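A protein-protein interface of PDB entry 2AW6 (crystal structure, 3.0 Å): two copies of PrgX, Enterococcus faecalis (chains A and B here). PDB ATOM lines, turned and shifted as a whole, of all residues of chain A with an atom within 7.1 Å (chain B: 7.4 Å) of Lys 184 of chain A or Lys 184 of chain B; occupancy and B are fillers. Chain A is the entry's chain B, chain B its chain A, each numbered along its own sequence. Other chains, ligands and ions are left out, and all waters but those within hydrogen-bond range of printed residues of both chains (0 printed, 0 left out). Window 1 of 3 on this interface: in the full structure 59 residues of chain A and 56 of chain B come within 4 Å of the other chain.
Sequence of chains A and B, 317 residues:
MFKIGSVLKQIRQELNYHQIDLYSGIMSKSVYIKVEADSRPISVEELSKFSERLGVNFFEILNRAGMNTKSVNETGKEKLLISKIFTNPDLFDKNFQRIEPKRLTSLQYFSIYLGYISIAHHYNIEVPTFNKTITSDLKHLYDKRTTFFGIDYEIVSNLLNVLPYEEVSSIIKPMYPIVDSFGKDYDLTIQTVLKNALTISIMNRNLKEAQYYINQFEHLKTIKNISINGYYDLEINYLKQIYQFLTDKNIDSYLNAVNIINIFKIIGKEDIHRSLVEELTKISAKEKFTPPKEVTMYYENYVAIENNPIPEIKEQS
Lys 184 of chain A touches just these residues of chain B: Lys 184 (3.4 Å) and Asp 185 (3.4 Å).
Of the printed residues of chain B, Asp 185 of chain A touches Lys 184.
Of chain A, only Lys 184 and Asp 185 come within 4 Å of Lys 184 of chain B.
Printed residues of chain A within 4 Å of Asp 185 of chain B: Lys 184 (3.4 Å).
Thr 189 of chain B touches none of the printed residues of chain A.
Ile 226 of chain B touches none of the printed residues of chain A.
The nearest residue of chain B that does not touch Lys 184 of chain A is Asn 63 of chain B (5.5 Å).
The nearest printed residue of chain A that does not touch Phe 182 of chain B is Lys 184 of chain A (9.7 Å).
Phe 59 of chain B touches Asn 63 of chain A (CZ to ND2, 3.5 Å).
Asn 63 of chain A touches Phe 182 of chain B (OD1 to C, 3.2 Å).
OD1 of Asn 63 of chain B touches C of Phe 182 of chain A (3.3 Å).
CB of Lys 184 of chain A touches NZ of Lys 184 of chain B, 3.4 Å away.
The backbone carbonyl oxygen of Phe 59 of chain B sits at hydrogen-bond distance from the side-chain amide nitrogen of Asn 63 of chain B.
The backbone carbonyl oxygen (O) of Asp 185 of chain B is in hydrogen-bond range of the side-chain hydroxyl (OG1) of Thr 189 of chain B, 3.3 Å away.
Asn 63 of chain A touches Phe 182 of chain B, and with the chains exchanged Phe 182 of chain A touches Asn 63 of chain B.
Asn 63 of chain A touches Gly 183 of chain B, and with the chains exchanged Gly 183 of chain A touches Asn 63 of chain B.
Lys 184 of chain A touches its own counterpart, Lys 184 of chain B.
Lys 184 of chain A touches Asp 185 of chain B, and with the chains exchanged Asp 185 of chain A touches Lys 184 of chain B.
Of the 8 pairs that touch across the chains among the printed residues, 7 have their exchanged pair printed and touching as well.
OD1 of Asn 63 of chain B lies within hydrogen-bond range of N of Gly 183 of chain A, at 2.9 Å.
N of Gly 183 of chain B lies within hydrogen-bond range of OD1 of Asn 63 of chain A (2.8 Å).
The side-chain amino group (NZ) of Lys 184 of chain B lies within salt-bridge range of the side-chain carboxylate (OD2) of Asp 185 of chain A.
The side-chain carboxylate of Asp 185 of chain B lies within salt-bridge range of the side-chain amino group of Lys 184 of chain A (3.4 Å).
Of the 16 printed residues of chain B, 6 touch a printed residue of chain A.
Printed residues of chain B that touch a printed residue of chain A: Phe 59, Asn 63, Phe 182, Gly 183, Lys 184 and Asp 185.
Hydrophobic or aromatic side chains of chain B that line the printed part of chain A: Phe 59.
Of the 14 printed residues of chain A, 5 touch a printed residue of chain B.
Among the printed residues, 8 pairs touch across the chains.
Among the printed residues, Asp or Glu carboxylates within 4 Å of a Lys or Arg side-chain nitrogen of the other chain: Lys 184 of chain A with Asp 185 of chain B and Asp 185 of chain A with Lys 184 of chain B.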
ATOM      1  N   ASN A  63     -28.217 -11.173 -12.457  1.00  0.00           N
ATOM      2  CA  ASN A  63     -29.361 -11.169 -13.361  1.00  0.00           C
ATOM      3  C   ASN A  63     -30.510 -10.348 -12.806  1.00  0.00           C
ATOM      4  O   ASN A  63     -31.077  -9.506 -13.511  1.00  0.00           O
ATOM      5  CB  ASN A  63     -29.796 -12.596 -13.701  1.00  0.00           C
ATOM      6  CG  ASN A  63     -28.865 -13.266 -14.711  1.00  0.00           C
ATOM      7  OD1 ASN A  63     -29.278 -14.157 -15.436  1.00  0.00           O
ATOM      8  ND2 ASN A  63     -27.611 -12.826 -14.767  1.00  0.00           N
ATOM      9  N   SER A 181     -14.392 -24.863 -20.245  1.00  0.00           N
ATOM     10  CA  SER A 181     -15.628 -24.104 -20.423  1.00  0.00           C
ATOM     11  C   SER A 181     -15.552 -22.753 -19.732  1.00  0.00           C
ATOM     12  O   SER A 181     -15.045 -22.650 -18.613  1.00  0.00           O
ATOM     13  CB  SER A 181     -16.814 -24.883 -19.869  1.00  0.00           C
ATOM     14  OG  SER A 181     -17.810 -24.005 -19.379  1.00  0.00           O
ATOM     15  N   PHE A 182     -16.067 -21.721 -20.394  1.00  0.00           N
ATOM     16  CA  PHE A 182     -16.098 -20.379 -19.814  1.00  0.00           C
ATOM     17  C   PHE A 182     -17.508 -19.772 -19.849  1.00  0.00           C
ATOM     18  O   PHE A 182     -17.713 -18.635 -20.306  1.00  0.00           O
ATOM     19  CB  PHE A 182     -15.088 -19.461 -20.505  1.00  0.00           C
ATOM     20  CG  PHE A 182     -13.663 -19.945 -20.432  1.00  0.00           C
ATOM     21  CD1 PHE A 182     -13.005 -20.041 -19.214  1.00  0.00           C
ATOM     22  CD2 PHE A 182     -12.972 -20.273 -21.589  1.00  0.00           C
ATOM     23  CE1 PHE A 182     -11.692 -20.473 -19.147  1.00  0.00           C
ATOM     24  CE2 PHE A 182     -11.661 -20.702 -21.531  1.00  0.00           C
ATOM     25  CZ  PHE A 182     -11.022 -20.807 -20.300  1.00  0.00           C
ATOM     26  N   GLY A 183     -18.476 -20.544 -19.362  1.00  0.00           N
ATOM     27  CA  GLY A 183     -19.860 -20.088 -19.278  1.00  0.00           C
ATOM     28  C   GLY A 183     -20.771 -20.851 -20.207  1.00  0.00           C
ATOM     29  O   GLY A 183     -20.300 -21.531 -21.119  1.00  0.00           O
ATOM     30  N   LYS A 184     -22.076 -20.727 -19.973  1.00  0.00           N
ATOM     31  CA  LYS A 184     -23.085 -21.381 -20.797  1.00  0.00           C
ATOM     32  C   LYS A 184     -23.134 -20.779 -22.209  1.00  0.00           C
ATOM     33  O   LYS A 184     -23.534 -21.454 -23.168  1.00  0.00           O
ATOM     34  CB  LYS A 184     -24.454 -21.312 -20.116  1.00  0.00           C
ATOM     35  CG  LYS A 184     -24.432 -21.623 -18.613  1.00  0.00           C
ATOM     36  CD  LYS A 184     -23.854 -23.006 -18.295  1.00  0.00           C
ATOM     37  CE  LYS A 184     -24.113 -23.412 -16.851  1.00  0.00           C
ATOM     38  NZ  LYS A 184     -25.563 -23.639 -16.581  1.00  0.00           N
ATOM     39  N   ASP A 185     -22.703 -19.520 -22.328  1.00  0.00           N
ATOM     40  CA  ASP A 185     -22.661 -18.831 -23.617  1.00  0.00           C
ATOM     41  C   ASP A 185     -21.465 -19.264 -24.468  1.00  0.00           C
ATOM     42  O   ASP A 185     -21.604 -19.582 -25.659  1.00  0.00           O
ATOM     43  CB  ASP A 185     -22.665 -17.322 -23.405  1.00  0.00           C
ATOM     44  CG  ASP A 185     -23.910 -16.851 -22.707  1.00  0.00           C
ATOM     45  OD1 ASP A 185     -23.795 -16.098 -21.722  1.00  0.00           O
ATOM     46  OD2 ASP A 185     -25.011 -17.255 -23.125  1.00  0.00           O
ATOM     47  N   TYR A 186     -20.287 -19.260 -23.853  1.00  0.00           N
ATOM     48  CA  TYR A 186     -19.097 -19.825 -24.468  1.00  0.00           C
ATOM     49  C   TYR A 186     -19.416 -21.238 -24.928  1.00  0.00           C
ATOM     50  O   TYR A 186     -19.054 -21.630 -26.035  1.00  0.00           O
ATOM     51  CB  TYR A 186     -17.969 -19.861 -23.449  1.00  0.00           C
ATOM     52  CG  TYR A 186     -16.654 -20.375 -23.959  1.00  0.00           C
ATOM     53  CD1 TYR A 186     -16.345 -21.728 -23.929  1.00  0.00           C
ATOM     54  CD2 TYR A 186     -15.696 -19.494 -24.432  1.00  0.00           C
ATOM     55  CE1 TYR A 186     -15.108 -22.186 -24.385  1.00  0.00           C
ATOM     56  CE2 TYR A 186     -14.468 -19.932 -24.886  1.00  0.00           C
ATOM     57  CZ  TYR A 186     -14.176 -21.269 -24.863  1.00  0.00           C
ATOM     58  OH  TYR A 186     -12.943 -21.658 -25.321  1.00  0.00           O
ATOM     59  N   ASP A 187     -20.110 -21.993 -24.075  1.00  0.00           N
ATOM     60  CA  ASP A 187     -20.467 -23.356 -24.403  1.00  0.00           C
ATOM     61  C   ASP A 187     -21.303 -23.336 -25.675  1.00  0.00           C
ATOM     62  O   ASP A 187     -21.061 -24.117 -26.593  1.00  0.00           O
ATOM     63  CB  ASP A 187     -21.222 -24.040 -23.248  1.00  0.00           C
ATOM     64  CG  ASP A 187     -20.342 -24.285 -22.009  1.00  0.00           C
ATOM     65  OD1 ASP A 187     -20.895 -24.321 -20.885  1.00  0.00           O
ATOM     66  OD2 ASP A 187     -19.109 -24.440 -22.140  1.00  0.00           O
ATOM     67  N   LEU A 188     -22.258 -22.415 -25.745  1.00  0.00           N
ATOM     68  CA  LEU A 188     -23.181 -22.367 -26.878  1.00  0.00           C
ATOM     69  C   LEU A 188     -22.467 -22.124 -28.214  1.00  0.00           C
ATOM     70  O   LEU A 188     -22.717 -22.823 -29.195  1.00  0.00           O
ATOM     71  CB  LEU A 188     -24.271 -21.312 -26.639  1.00  0.00           C
ATOM     72  CG  LEU A 188     -25.423 -21.284 -27.637  1.00  0.00           C
ATOM     73  CD1 LEU A 188     -26.333 -22.469 -27.404  1.00  0.00           C
ATOM     74  CD2 LEU A 188     -26.183 -20.003 -27.486  1.00  0.00           C
ATOM     75  N   THR A 189     -21.571 -21.145 -28.241  1.00  0.00           N
ATOM     76  CA  THR A 189     -20.942 -20.724 -29.488  1.00  0.00           C
ATOM     77  C   THR A 189     -19.934 -21.756 -29.995  1.00  0.00           C
ATOM     78  O   THR A 189     -19.898 -22.051 -31.186  1.00  0.00           O
ATOM     79  CB  THR A 189     -20.312 -19.332 -29.348  1.00  0.00           C
ATOM     80  OG1 THR A 189     -19.265 -19.383 -28.377  1.00  0.00           O
ATOM     81  CG2 THR A 189     -21.357 -18.331 -28.873  1.00  0.00           C
ATOM     82  N   GLN A 191     -20.121 -24.883 -29.561  1.00  0.00           N
ATOM     83  CA  GLN A 191     -20.947 -25.918 -30.153  1.00  0.00           C
ATOM     84  C   GLN A 191     -21.525 -25.499 -31.494  1.00  0.00           C
ATOM     85  O   GLN A 191     -21.624 -26.329 -32.382  1.00  0.00           O
ATOM     86  CB  GLN A 191     -22.082 -26.327 -29.224  1.00  0.00           C
ATOM     87  CG  GLN A 191     -21.632 -27.023 -27.983  1.00  0.00           C
ATOM     88  CD  GLN A 191     -22.775 -27.335 -27.062  1.00  0.00           C
ATOM     89  OE1 GLN A 191     -23.698 -28.061 -27.424  1.00  0.00           O
ATOM     90  NE2 GLN A 191     -22.725 -26.786 -25.858  1.00  0.00           N
ATOM     91  N   ASN A 225     -17.611 -29.393 -16.552  1.00  0.00           N
ATOM     92  CA  ASN A 225     -18.366 -28.138 -16.449  1.00  0.00           C
ATOM     93  C   ASN A 225     -19.017 -27.685 -17.760  1.00  0.00           C
ATOM     94  O   ASN A 225     -19.833 -26.749 -17.755  1.00  0.00           O
ATOM     95  CB  ASN A 225     -17.526 -27.001 -15.828  1.00  0.00           C
ATOM     96  CG  ASN A 225     -17.692 -26.894 -14.314  1.00  0.00           C
ATOM     97  OD1 ASN A 225     -18.769 -27.150 -13.768  1.00  0.00           O
ATOM     98  ND2 ASN A 225     -16.623 -26.488 -13.631  1.00  0.00           N
ATOM     99  N   ILE A 226     -18.670 -28.346 -18.870  1.00  0.00           N
ATOM    100  CA  ILE A 226     -19.245 -28.024 -20.187  1.00  0.00           C
ATOM    101  C   ILE A 226     -20.752 -28.259 -20.189  1.00  0.00           C
ATOM    102  O   ILE A 226     -21.222 -29.311 -19.753  1.00  0.00           O
ATOM    103  CB  ILE A 226     -18.614 -28.861 -21.332  1.00  0.00           C
ATOM    104  CG1 ILE A 226     -18.568 -28.049 -22.622  1.00  0.00           C
ATOM    105  CG2 ILE A 226     -19.361 -30.191 -21.565  1.00  0.00           C
ATOM    106  CD1 ILE A 226     -17.287 -27.279 -22.790  1.00  0.00           C
ATOM    107  N   SER A 227     -21.516 -27.288 -20.673  1.00  0.00           N
ATOM    108  CA  SER A 227     -22.961 -27.436 -20.677  1.00  0.00           C
ATOM    109  C   SER A 227     -23.453 -27.705 -22.088  1.00  0.00           C
ATOM    110  O   SER A 227     -23.789 -26.773 -22.810  1.00  0.00           O
ATOM    111  CB  SER A 227     -23.621 -26.204 -20.077  1.00  0.00           C
ATOM    112  OG  SER A 227     -24.933 -26.516 -19.662  1.00  0.00           O
ATOM    113  N   PHE B  59     -19.776 -12.090 -18.414  1.00  0.00           N
ATOM    114  CA  PHE B  59     -19.805 -13.310 -17.627  1.00  0.00           C
ATOM    115  C   PHE B  59     -18.665 -14.257 -17.982  1.00  0.00           C
ATOM    116  O   PHE B  59     -18.174 -14.990 -17.118  1.00  0.00           O
ATOM    117  CB  PHE B  59     -21.156 -13.998 -17.772  1.00  0.00           C
ATOM    118  CG  PHE B  59     -22.261 -13.299 -17.046  1.00  0.00           C
ATOM    119  CD1 PHE B  59     -22.607 -13.683 -15.758  1.00  0.00           C
ATOM    120  CD2 PHE B  59     -22.947 -12.251 -17.639  1.00  0.00           C
ATOM    121  CE1 PHE B  59     -23.621 -13.045 -15.075  1.00  0.00           C
ATOM    122  CE2 PHE B  59     -23.962 -11.604 -16.960  1.00  0.00           C
ATOM    123  CZ  PHE B  59     -24.298 -12.006 -15.674  1.00  0.00           C
ATOM    124  N   ASN B  63     -15.951 -16.030 -15.593  1.00  0.00           N
ATOM    125  CA  ASN B  63     -15.545 -17.424 -15.626  1.00  0.00           C
ATOM    126  C   ASN B  63     -14.039 -17.557 -15.708  1.00  0.00           C
ATOM    127  O   ASN B  63     -13.421 -18.282 -14.925  1.00  0.00           O
ATOM    128  CB  ASN B  63     -16.193 -18.146 -16.800  1.00  0.00           C
ATOM    129  CG  ASN B  63     -17.592 -18.598 -16.490  1.00  0.00           C
ATOM    130  OD1 ASN B  63     -17.896 -19.783 -16.587  1.00  0.00           O
ATOM    131  ND2 ASN B  63     -18.454 -17.661 -16.098  1.00  0.00           N
ATOM    132  N   SER B 181     -36.885 -15.025 -16.242  1.00  0.00           N
ATOM    133  CA  SER B 181     -35.669 -15.828 -16.100  1.00  0.00           C
ATOM    134  C   SER B 181     -34.524 -15.056 -15.417  1.00  0.00           C
ATOM    135  O   SER B 181     -34.298 -13.888 -15.707  1.00  0.00           O
ATOM    136  CB  SER B 181     -35.220 -16.345 -17.465  1.00  0.00           C
ATOM    137  OG  SER B 181     -33.918 -16.884 -17.374  1.00  0.00           O
ATOM    138  N   PHE B 182     -33.814 -15.715 -14.509  1.00  0.00           N
ATOM    139  CA  PHE B 182     -32.687 -15.093 -13.796  1.00  0.00           C
ATOM    140  C   PHE B 182     -31.408 -15.944 -13.915  1.00  0.00           C
ATOM    141  O   PHE B 182     -30.731 -16.251 -12.920  1.00  0.00           O
ATOM    142  CB  PHE B 182     -33.035 -14.809 -12.325  1.00  0.00           C
ATOM    143  CG  PHE B 182     -34.240 -13.927 -12.141  1.00  0.00           C
ATOM    144  CD1 PHE B 182     -34.203 -12.581 -12.505  1.00  0.00           C
ATOM    145  CD2 PHE B 182     -35.418 -14.441 -11.593  1.00  0.00           C
ATOM    146  CE1 PHE B 182     -35.317 -11.766 -12.325  1.00  0.00           C
ATOM    147  CE2 PHE B 182     -36.543 -13.627 -11.408  1.00  0.00           C
ATOM    148  CZ  PHE B 182     -36.486 -12.290 -11.777  1.00  0.00           C
ATOM    149  N   GLY B 183     -31.101 -16.324 -15.152  1.00  0.00           N
ATOM    150  CA  GLY B 183     -29.898 -17.071 -15.461  1.00  0.00           C
ATOM    151  C   GLY B 183     -30.194 -18.489 -15.883  1.00  0.00           C
ATOM    152  O   GLY B 183     -31.319 -18.974 -15.702  1.00  0.00           O
ATOM    153  N   LYS B 184     -29.175 -19.159 -16.427  1.00  0.00           N
ATOM    154  CA  LYS B 184     -29.307 -20.541 -16.890  1.00  0.00           C
ATOM    155  C   LYS B 184     -29.462 -21.522 -15.733  1.00  0.00           C
ATOM    156  O   LYS B 184     -30.010 -22.611 -15.921  1.00  0.00           O
ATOM    157  CB  LYS B 184     -28.123 -20.954 -17.772  1.00  0.00           C
ATOM    158  CG  LYS B 184     -27.640 -19.878 -18.748  1.00  0.00           C
ATOM    159  CD  LYS B 184     -28.592 -19.655 -19.918  1.00  0.00           C
ATOM    160  CE  LYS B 184     -28.001 -18.688 -20.938  1.00  0.00           C
ATOM    161  NZ  LYS B 184     -26.774 -19.230 -21.589  1.00  0.00           N
ATOM    162  N   ASP B 185     -28.993 -21.134 -14.544  1.00  0.00           N
ATOM    163  CA  ASP B 185     -29.111 -21.968 -13.346  1.00  0.00           C
ATOM    164  C   ASP B 185     -30.502 -21.900 -12.742  1.00  0.00           C
ATOM    165  O   ASP B 185     -31.110 -22.929 -12.432  1.00  0.00           O
ATOM    166  CB  ASP B 185     -28.054 -21.588 -12.318  1.00  0.00           C
ATOM    167  CG  ASP B 185     -26.652 -21.869 -12.809  1.00  0.00           C
ATOM    168  OD1 ASP B 185     -25.799 -20.963 -12.716  1.00  0.00           O
ATOM    169  OD2 ASP B 185     -26.403 -22.989 -13.306  1.00  0.00           O
ATOM    170  N   TYR B 186     -31.002 -20.680 -12.586  1.00  0.00           N
ATOM    171  CA  TYR B 186     -32.391 -20.444 -12.220  1.00  0.00           C
ATOM    172  C   TYR B 186     -33.312 -21.200 -13.172  1.00  0.00           C
ATOM    173  O   TYR B 186     -34.285 -21.838 -12.752  1.00  0.00           O
ATOM    174  CB  TYR B 186     -32.671 -18.960 -12.295  1.00  0.00           C
ATOM    175  CG  TYR B 186     -34.088 -18.555 -11.981  1.00  0.00           C
ATOM    176  CD1 TYR B 186     -34.967 -18.206 -13.002  1.00  0.00           C
ATOM    177  CD2 TYR B 186     -34.547 -18.478 -10.663  1.00  0.00           C
ATOM    178  CE1 TYR B 186     -36.266 -17.802 -12.729  1.00  0.00           C
ATOM    179  CE2 TYR B 186     -35.859 -18.075 -10.377  1.00  0.00           C
ATOM    180  CZ  TYR B 186     -36.705 -17.738 -11.424  1.00  0.00           C
ATOM    181  OH  TYR B 186     -37.993 -17.332 -11.189  1.00  0.00           O
ATOM    182  N   ASP B 187     -32.981 -21.132 -14.459  1.00  0.00           N
ATOM    183  CA  ASP B 187     -33.704 -21.874 -15.476  1.00  0.00           C
ATOM    184  C   ASP B 187     -33.706 -23.363 -15.146  1.00  0.00           C
ATOM    185  O   ASP B 187     -34.749 -24.021 -15.246  1.00  0.00           O
ATOM    186  CB  ASP B 187     -33.091 -21.632 -16.859  1.00  0.00           C
ATOM    187  CG  ASP B 187     -33.378 -20.238 -17.392  1.00  0.00           C
ATOM    188  OD1 ASP B 187     -34.332 -19.582 -16.920  1.00  0.00           O
ATOM    189  OD2 ASP B 187     -32.640 -19.797 -18.294  1.00  0.00           O
ATOM    190  N   LEU B 188     -32.545 -23.880 -14.727  1.00  0.00           N
ATOM    191  CA  LEU B 188     -32.383 -25.317 -14.501  1.00  0.00           C
ATOM    192  C   LEU B 188     -33.274 -25.794 -13.362  1.00  0.00           C
ATOM    193  O   LEU B 188     -34.023 -26.763 -13.510  1.00  0.00           O
ATOM    194  CB  LEU B 188     -30.929 -25.668 -14.182  1.00  0.00           C
ATOM    195  CG  LEU B 188     -30.286 -27.008 -14.593  1.00  0.00           C
ATOM    196  CD1 LEU B 188     -29.324 -27.432 -13.497  1.00  0.00           C
ATOM    197  CD2 LEU B 188     -31.250 -28.147 -14.892  1.00  0.00           C
ATOM    198  N   THR B 189     -33.194 -25.104 -12.232  1.00  0.00           N
ATOM    199  CA  THR B 189     -33.883 -25.536 -11.031  1.00  0.00           C
ATOM    200  C   THR B 189     -35.406 -25.449 -11.171  1.00  0.00           C
ATOM    201  O   THR B 189     -36.114 -26.408 -10.821  1.00  0.00           O
ATOM    202  CB  THR B 189     -33.413 -24.749  -9.818  1.00  0.00           C
ATOM    203  OG1 THR B 189     -33.411 -23.359 -10.142  1.00  0.00           O
ATOM    204  CG2 THR B 189     -32.014 -25.151  -9.443  1.00  0.00           C
ATOM    205  N   GLN B 191     -37.062 -25.739 -13.825  1.00  0.00           N
ATOM    206  CA  GLN B 191     -37.387 -26.881 -14.684  1.00  0.00           C
ATOM    207  C   GLN B 191     -37.326 -28.200 -13.918  1.00  0.00           C
ATOM    208  O   GLN B 191     -38.183 -29.064 -14.091  1.00  0.00           O
ATOM    209  CB  GLN B 191     -36.481 -26.926 -15.916  1.00  0.00           C
ATOM    210  CG  GLN B 191     -36.884 -25.965 -17.017  1.00  0.00           C
ATOM    211  CD  GLN B 191     -35.874 -25.901 -18.151  1.00  0.00           C
ATOM    212  OE1 GLN B 191     -35.952 -26.666 -19.111  1.00  0.00           O
ATOM    213  NE2 GLN B 191     -34.928 -24.974 -18.052  1.00  0.00           N
ATOM    214  N   ASN B 225     -36.145 -15.116 -22.888  1.00  0.00           N
ATOM    215  CA  ASN B 225     -34.817 -15.284 -22.269  1.00  0.00           C
ATOM    216  C   ASN B 225     -34.623 -16.606 -21.536  1.00  0.00           C
ATOM    217  O   ASN B 225     -33.498 -16.950 -21.157  1.00  0.00           O
ATOM    218  CB  ASN B 225     -34.468 -14.117 -21.323  1.00  0.00           C
ATOM    219  CG  ASN B 225     -33.634 -13.035 -21.990  1.00  0.00           C
ATOM    220  OD1 ASN B 225     -33.252 -13.146 -23.156  1.00  0.00           O
ATOM    221  ND2 ASN B 225     -33.343 -11.976 -21.240  1.00  0.00           N
ATOM    222  N   ILE B 226     -35.710 -17.345 -21.329  1.00  0.00           N
ATOM    223  CA  ILE B 226     -35.624 -18.602 -20.590  1.00  0.00           C
ATOM    224  C   ILE B 226     -34.884 -19.660 -21.391  1.00  0.00           C
ATOM    225  O   ILE B 226     -35.090 -19.810 -22.596  1.00  0.00           O
ATOM    226  CB  ILE B 226     -36.996 -19.111 -20.111  1.00  0.00           C
ATOM    227  CG1 ILE B 226     -36.815 -20.089 -18.954  1.00  0.00           C
ATOM    228  CG2 ILE B 226     -37.790 -19.716 -21.267  1.00  0.00           C
ATOM    229  CD1 ILE B 226     -38.060 -20.290 -18.154  1.00  0.00           C
ATOM    230  N   SER B 227     -34.002 -20.371 -20.710  1.00  0.00           N
ATOM    231  CA  SER B 227     -33.141 -21.336 -21.358  1.00  0.00           C
ATOM    232  C   SER B 227     -33.610 -22.768 -21.073  1.00  0.00           C
ATOM    233  O   SER B 227     -33.119 -23.429 -20.152  1.00  0.00           O
ATOM    234  CB  SER B 227     -31.714 -21.119 -20.879  1.00  0.00           C
ATOM    235  OG  SER B 227     -30.815 -21.856 -21.668  1.00  0.00           O
ATOM    236  N   ILE B 228     -34.574 -23.232 -21.863  1.00  0.00           N
ATOM    237  CA  ILE B 228     -35.122 -24.573 -21.736  1.00  0.00           C
ATOM    238  C   ILE B 228     -34.022 -25.613 -21.895  1.00  0.00           C
ATOM    239  O   ILE B 228     -33.165 -25.524 -22.792  1.00  0.00           O
ATOM    240  CB  ILE B 228     -36.211 -24.831 -22.805  1.00  0.00           C
ATOM    241  CG1 ILE B 228     -37.318 -23.770 -22.717  1.00  0.00           C
ATOM    242  CG2 ILE B 228     -36.769 -26.252 -22.711  1.00  0.00           C
ATOM    243  CD1 ILE B 228     -38.091 -23.733 -21.392  1.00  0.00           C
